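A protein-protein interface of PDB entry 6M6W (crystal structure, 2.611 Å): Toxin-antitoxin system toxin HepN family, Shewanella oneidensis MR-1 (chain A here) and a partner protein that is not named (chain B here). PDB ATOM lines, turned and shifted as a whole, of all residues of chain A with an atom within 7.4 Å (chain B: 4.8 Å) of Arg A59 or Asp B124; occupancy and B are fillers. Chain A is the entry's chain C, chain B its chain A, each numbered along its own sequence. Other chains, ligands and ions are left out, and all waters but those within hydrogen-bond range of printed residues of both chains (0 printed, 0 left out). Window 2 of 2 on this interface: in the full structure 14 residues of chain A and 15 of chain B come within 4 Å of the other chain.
The side-chain carboxylate (OD2) of Asp B124 is in salt-bridge range of the guanidinium group (NH1) of Arg A59 (3.4 Å).
O of Ala A54 lies within hydrogen-bond range of ND2 of Asn A58. The backbone NH (N) of Leu A63 lies within hydrogen-bond range of the backbone carbonyl oxygen (O) of Asn A58, 3.1 Å away.
Among the printed residues, merely in contact across the chains: Asn A55 with Ile B121, Arg A59 with Ala B120, Arg A59 with Ile B121, Gly A64 with Ile B121 and Asn A58 with Ile B121.
Printed residues of chain B within 4 Å of Asn A55: Ile B121. Of the printed residues of chain B, Asn A58 touches Ile B121 (3.8 Å). Arg A59 touches three residues of chain B. Gln A61 touches none of the printed residues of chain B. Gln A62 touches none of the printed residues of chain B. Of the printed residues of chain B, Gly A64 touches Ile B121 (3.7 Å). Of the printed residues of chain A, Ala B120 touches Arg A59 (3.7 Å). Printed residues of chain A within 4 Å of Ile B121: Asn A55, Asn A58, Arg A59 and Gly A64. Asp B124 touches just one residue of chain A: Arg A59.
Printed residues of chain B that touch a printed residue of chain A: Ala B120, Ile B121 and Asp B124. Hydrophobic or aromatic side chains of chain B within 4 Å of the printed part of chain A: Ala B120 and Ile B121. Among the printed residues, 6 pairs touch across the chains. Among the printed residues, Asp or Glu carboxylates within 4 Å of a Lys or Arg side-chain nitrogen of the other chain: Arg A59 with Asp B124.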
ATOM      1  N   ILE A   4      26.503   1.390 -11.185  1.00  0.00           N
ATOM      2  CA  ILE A   4      25.732   1.862 -12.311  1.00  0.00           C
ATOM      3  C   ILE A   4      24.816   3.030 -12.048  1.00  0.00           C
ATOM      4  O   ILE A   4      24.461   3.736 -12.963  1.00  0.00           O
ATOM      5  CB  ILE A   4      24.871   0.740 -12.871  1.00  0.00           C
ATOM      6  CG1 ILE A   4      24.013   1.276 -13.994  1.00  0.00           C
ATOM      7  CG2 ILE A   4      23.997   0.168 -11.783  1.00  0.00           C
ATOM      8  CD1 ILE A   4      24.759   1.373 -15.302  1.00  0.00           C
ATOM      9  N   ASP A  52      16.698   3.905 -16.523  1.00  0.00           N
ATOM     10  CA  ASP A  52      17.692   2.909 -16.136  1.00  0.00           C
ATOM     11  C   ASP A  52      17.890   2.882 -14.626  1.00  0.00           C
ATOM     12  O   ASP A  52      17.996   1.804 -14.032  1.00  0.00           O
ATOM     13  CB  ASP A  52      19.020   3.180 -16.845  1.00  0.00           C
ATOM     14  CG  ASP A  52      18.924   3.031 -18.349  1.00  0.00           C
ATOM     15  OD1 ASP A  52      17.829   2.693 -18.845  1.00  0.00           O
ATOM     16  OD2 ASP A  52      19.942   3.258 -19.038  1.00  0.00           O
ATOM     17  N   ILE A  53      17.959   4.055 -13.988  1.00  0.00           N
ATOM     18  CA  ILE A  53      17.988   4.101 -12.527  1.00  0.00           C
ATOM     19  C   ILE A  53      16.755   3.419 -11.945  1.00  0.00           C
ATOM     20  O   ILE A  53      16.855   2.580 -11.041  1.00  0.00           O
ATOM     21  CB  ILE A  53      18.113   5.552 -12.026  1.00  0.00           C
ATOM     22  CG1 ILE A  53      19.501   6.112 -12.342  1.00  0.00           C
ATOM     23  CG2 ILE A  53      17.831   5.626 -10.531  1.00  0.00           C
ATOM     24  CD1 ILE A  53      19.621   7.604 -12.115  1.00  0.00           C
ATOM     25  N   ALA A  54      15.573   3.770 -12.457  1.00  0.00           N
ATOM     26  CA  ALA A  54      14.330   3.224 -11.918  1.00  0.00           C
ATOM     27  C   ALA A  54      14.268   1.711 -12.083  1.00  0.00           C
ATOM     28  O   ALA A  54      13.948   0.986 -11.133  1.00  0.00           O
ATOM     29  CB  ALA A  54      13.132   3.892 -12.594  1.00  0.00           C
ATOM     30  N   ASN A  55      14.572   1.213 -13.286  1.00  0.00           N
ATOM     31  CA  ASN A  55      14.554  -0.229 -13.517  1.00  0.00           C
ATOM     32  C   ASN A  55      15.610  -0.955 -12.699  1.00  0.00           C
ATOM     33  O   ASN A  55      15.388  -2.096 -12.278  1.00  0.00           O
ATOM     34  CB  ASN A  55      14.733  -0.543 -15.001  1.00  0.00           C
ATOM     35  CG  ASN A  55      13.469  -0.321 -15.800  1.00  0.00           C
ATOM     36  OD1 ASN A  55      12.366  -0.395 -15.261  1.00  0.00           O
ATOM     37  ND2 ASN A  55      13.620  -0.060 -17.093  1.00  0.00           N
ATOM     38  N   HIS A  56      16.764  -0.328 -12.467  1.00  0.00           N
ATOM     39  CA  HIS A  56      17.788  -0.988 -11.667  1.00  0.00           C
ATOM     40  C   HIS A  56      17.314  -1.178 -10.233  1.00  0.00           C
ATOM     41  O   HIS A  56      17.578  -2.218  -9.618  1.00  0.00           O
ATOM     42  CB  HIS A  56      19.092  -0.195 -11.708  1.00  0.00           C
ATOM     43  CG  HIS A  56      20.185  -0.806 -10.893  1.00  0.00           C
ATOM     44  ND1 HIS A  56      20.478  -0.391  -9.613  1.00  0.00           N
ATOM     45  CD2 HIS A  56      21.036  -1.824 -11.162  1.00  0.00           C
ATOM     46  CE1 HIS A  56      21.473  -1.114  -9.134  1.00  0.00           C
ATOM     47  NE2 HIS A  56      21.832  -1.991 -10.054  1.00  0.00           N
ATOM     48  N   ILE A  57      16.615  -0.183  -9.687  1.00  0.00           N
ATOM     49  CA  ILE A  57      16.024  -0.309  -8.360  1.00  0.00           C
ATOM     50  C   ILE A  57      14.914  -1.351  -8.383  1.00  0.00           C
ATOM     51  O   ILE A  57      14.783  -2.168  -7.462  1.00  0.00           O
ATOM     52  CB  ILE A  57      15.512   1.061  -7.882  1.00  0.00           C
ATOM     53  CG1 ILE A  57      16.682   2.042  -7.763  1.00  0.00           C
ATOM     54  CG2 ILE A  57      14.767   0.918  -6.559  1.00  0.00           C
ATOM     55  CD1 ILE A  57      16.276   3.482  -7.627  1.00  0.00           C
ATOM     56  N   ASN A  58      14.086  -1.318  -9.434  1.00  0.00           N
ATOM     57  CA  ASN A  58      13.035  -2.317  -9.598  1.00  0.00           C
ATOM     58  C   ASN A  58      13.609  -3.720  -9.539  1.00  0.00           C
ATOM     59  O   ASN A  58      13.029  -4.615  -8.916  1.00  0.00           O
ATOM     60  CB  ASN A  58      12.305  -2.114 -10.926  1.00  0.00           C
ATOM     61  CG  ASN A  58      11.508  -0.829 -10.969  1.00  0.00           C
ATOM     62  OD1 ASN A  58      10.863  -0.522 -11.971  1.00  0.00           O
ATOM     63  ND2 ASN A  58      11.552  -0.068  -9.884  1.00  0.00           N
ATOM     64  N   ARG A  59      14.766  -3.917 -10.163  1.00  0.00           N
ATOM     65  CA  ARG A  59      15.365  -5.238 -10.262  1.00  0.00           C
ATOM     66  C   ARG A  59      15.987  -5.685  -8.943  1.00  0.00           C
ATOM     67  O   ARG A  59      15.815  -6.841  -8.538  1.00  0.00           O
ATOM     68  CB  ARG A  59      16.398  -5.227 -11.388  1.00  0.00           C
ATOM     69  CG  ARG A  59      17.001  -6.564 -11.711  1.00  0.00           C
ATOM     70  CD  ARG A  59      18.424  -6.608 -11.207  1.00  0.00           C
ATOM     71  NE  ARG A  59      19.251  -5.576 -11.822  1.00  0.00           N
ATOM     72  CZ  ARG A  59      20.047  -5.780 -12.866  1.00  0.00           C
ATOM     73  NH1 ARG A  59      20.121  -6.981 -13.424  1.00  0.00           N
ATOM     74  NH2 ARG A  59      20.766  -4.780 -13.355  1.00  0.00           N
ATOM     75  N   GLN A  60      16.704  -4.792  -8.253  1.00  0.00           N
ATOM     76  CA  GLN A  60      17.382  -5.199  -7.025  1.00  0.00           C
ATOM     77  C   GLN A  60      16.399  -5.452  -5.889  1.00  0.00           C
ATOM     78  O   GLN A  60      16.670  -6.280  -5.010  1.00  0.00           O
ATOM     79  CB  GLN A  60      18.419  -4.149  -6.611  1.00  0.00           C
ATOM     80  CG  GLN A  60      17.866  -2.922  -5.893  1.00  0.00           C
ATOM     81  CD  GLN A  60      18.878  -1.796  -5.795  1.00  0.00           C
ATOM     82  OE1 GLN A  60      20.010  -1.926  -6.261  1.00  0.00           O
ATOM     83  NE2 GLN A  60      18.476  -0.681  -5.192  1.00  0.00           N
ATOM     84  N   GLN A  61      15.257  -4.764  -5.882  1.00  0.00           N
ATOM     85  CA  GLN A  61      14.244  -4.981  -4.859  1.00  0.00           C
ATOM     86  C   GLN A  61      13.034  -5.742  -5.386  1.00  0.00           C
ATOM     87  O   GLN A  61      12.065  -5.927  -4.642  1.00  0.00           O
ATOM     88  CB  GLN A  61      13.812  -3.644  -4.246  1.00  0.00           C
ATOM     89  CG  GLN A  61      14.958  -2.698  -3.943  1.00  0.00           C
ATOM     90  CD  GLN A  61      14.541  -1.503  -3.109  1.00  0.00           C
ATOM     91  OE1 GLN A  61      13.533  -1.541  -2.406  1.00  0.00           O
ATOM     92  NE2 GLN A  61      15.322  -0.431  -3.184  1.00  0.00           N
ATOM     93  N   GLN A  62      13.062  -6.172  -6.652  1.00  0.00           N
ATOM     94  CA  GLN A  62      12.086  -7.113  -7.216  1.00  0.00           C
ATOM     95  C   GLN A  62      10.648  -6.619  -7.055  1.00  0.00           C
ATOM     96  O   GLN A  62       9.775  -7.325  -6.547  1.00  0.00           O
ATOM     97  CB  GLN A  62      12.246  -8.514  -6.618  1.00  0.00           C
ATOM     98  CG  GLN A  62      13.610  -9.139  -6.841  1.00  0.00           C
ATOM     99  CD  GLN A  62      13.621 -10.614  -6.494  1.00  0.00           C
ATOM    100  OE1 GLN A  62      13.099 -11.432  -7.252  1.00  0.00           O
ATOM    101  NE2 GLN A  62      14.196 -10.965  -5.347  1.00  0.00           N
ATOM    102  N   LEU A  63      10.399  -5.392  -7.511  1.00  0.00           N
ATOM    103  CA  LEU A  63       9.080  -4.787  -7.386  1.00  0.00           C
ATOM    104  C   LEU A  63       8.142  -5.132  -8.540  1.00  0.00           C
ATOM    105  O   LEU A  63       6.932  -4.912  -8.414  1.00  0.00           O
ATOM    106  CB  LEU A  63       9.208  -3.261  -7.244  1.00  0.00           C
ATOM    107  CG  LEU A  63      10.146  -2.658  -6.176  1.00  0.00           C
ATOM    108  CD1 LEU A  63      11.594  -2.779  -6.568  1.00  0.00           C
ATOM    109  CD2 LEU A  63       9.822  -1.182  -5.916  1.00  0.00           C
ATOM    110  N   GLY A  64       8.639  -5.696  -9.627  1.00  0.00           N
ATOM    111  CA  GLY A  64       7.754  -6.097 -10.704  1.00  0.00           C
ATOM    112  C   GLY A  64       8.415  -5.967 -12.064  1.00  0.00           C
ATOM    113  O   GLY A  64       9.563  -5.545 -12.190  1.00  0.00           O
ATOM    114  N   ALA B 120      17.077  -6.951 -18.457  1.00  0.00           N
ATOM    115  CA  ALA B 120      17.756  -7.374 -17.237  1.00  0.00           C
ATOM    116  C   ALA B 120      16.750  -7.778 -16.165  1.00  0.00           C
ATOM    117  O   ALA B 120      17.001  -8.700 -15.381  1.00  0.00           O
ATOM    118  CB  ALA B 120      18.663  -6.255 -16.727  1.00  0.00           C
ATOM    119  N   ILE B 121      15.602  -7.099 -16.116  1.00  0.00           N
ATOM    120  CA  ILE B 121      14.563  -7.462 -15.155  1.00  0.00           C
ATOM    121  C   ILE B 121      13.936  -8.809 -15.504  1.00  0.00           C
ATOM    122  O   ILE B 121      13.789  -9.678 -14.636  1.00  0.00           O
ATOM    123  CB  ILE B 121      13.507  -6.346 -15.055  1.00  0.00           C
ATOM    124  CG1 ILE B 121      14.068  -5.169 -14.253  1.00  0.00           C
ATOM    125  CG2 ILE B 121      12.223  -6.870 -14.436  1.00  0.00           C
ATOM    126  CD1 ILE B 121      13.105  -4.016 -14.096  1.00  0.00           C
ATOM    127  N   ILE B 122      13.545  -9.010 -16.768  1.00  0.00           N
ATOM    128  CA  ILE B 122      12.935 -10.289 -17.132  1.00  0.00           C
ATOM    129  C   ILE B 122      13.930 -11.431 -16.941  1.00  0.00           C
ATOM    130  O   ILE B 122      13.557 -12.525 -16.501  1.00  0.00           O
ATOM    131  CB  ILE B 122      12.330 -10.249 -18.554  1.00  0.00           C
ATOM    132  CG1 ILE B 122      13.382 -10.383 -19.655  1.00  0.00           C
ATOM    133  CG2 ILE B 122      11.499  -8.984 -18.743  1.00  0.00           C
ATOM    134  CD1 ILE B 122      12.779 -10.624 -21.031  1.00  0.00           C
ATOM    135  N   ASP B 123      15.203 -11.207 -17.286  1.00  0.00           N
ATOM    136  CA  ASP B 123      16.205 -12.255 -17.095  1.00  0.00           C
ATOM    137  C   ASP B 123      16.322 -12.654 -15.627  1.00  0.00           C
ATOM    138  O   ASP B 123      16.459 -13.842 -15.310  1.00  0.00           O
ATOM    139  CB  ASP B 123      17.563 -11.809 -17.636  1.00  0.00           C
ATOM    140  CG  ASP B 123      17.633 -11.854 -19.152  1.00  0.00           C
ATOM    141  OD1 ASP B 123      16.828 -12.588 -19.766  1.00  0.00           O
ATOM    142  OD2 ASP B 123      18.507 -11.173 -19.728  1.00  0.00           O
ATOM    143  N   ASP B 124      16.272 -11.681 -14.714  1.00  0.00           N
ATOM    144  CA  ASP B 124      16.447 -12.017 -13.303  1.00  0.00           C
ATOM    145  C   ASP B 124      15.228 -12.735 -12.741  1.00  0.00           C
ATOM    146  O   ASP B 124      15.363 -13.565 -11.833  1.00  0.00           O
ATOM    147  CB  ASP B 124      16.750 -10.774 -12.469  1.00  0.00           C
ATOM    148  CG  ASP B 124      18.176 -10.293 -12.639  1.00  0.00           C
ATOM    149  OD1 ASP B 124      18.828 -10.702 -13.621  1.00  0.00           O
ATOM    150  OD2 ASP B 124      18.664  -9.547 -11.767  1.00  0.00           O
ATOM    151  N   VAL B 125      14.035 -12.436 -13.260  1.00  0.00           N
ATOM    152  CA  VAL B 125      12.821 -13.073 -12.756  1.00  0.00           C
ATOM    153  C   VAL B 125      12.584 -14.434 -13.389  1.00  0.00           C
ATOM    154  O   VAL B 125      11.822 -15.241 -12.840  1.00  0.00           O
ATOM    155  CB  VAL B 125      11.639 -12.104 -12.964  1.00  0.00           C
ATOM    156  CG1 VAL B 125      10.287 -12.785 -12.762  1.00  0.00           C
ATOM    157  CG2 VAL B 125      11.762 -10.923 -12.015  1.00  0.00           C
ATOM    158  N   MET B 126      13.283 -14.759 -14.476  1.00  0.00           N
ATOM    159  CA  MET B 126      13.162 -16.079 -15.081  1.00  0.00           C
ATOM    160  C   MET B 126      14.429 -16.908 -14.903  1.00  0.00           C
ATOM    161  O   MET B 126      14.710 -17.790 -15.724  1.00  0.00           O
ATOM    162  CB  MET B 126      12.814 -15.954 -16.566  1.00  0.00           C
ATOM    163  CG  MET B 126      11.528 -15.189 -16.840  1.00  0.00           C
ATOM    164  SD  MET B 126      10.051 -16.212 -16.865  1.00  0.00           S
ATOM    165  CE  MET B 126      10.331 -17.142 -18.368  1.00  0.00           C
ATOM    166  N   ALA B 127      15.189 -16.647 -13.840  1.00  0.00           N
ATOM    167  CA  ALA B 127      16.300 -17.495 -13.401  1.00  0.00           C
ATOM    168  C   ALA B 127      17.284 -17.837 -14.519  1.00  0.00           C
ATOM    169  O   ALA B 127      17.439 -17.087 -15.481  1.00  0.00           O
ATOM    170  CB  ALA B 127      15.759 -18.770 -12.774  1.00  0.00           C
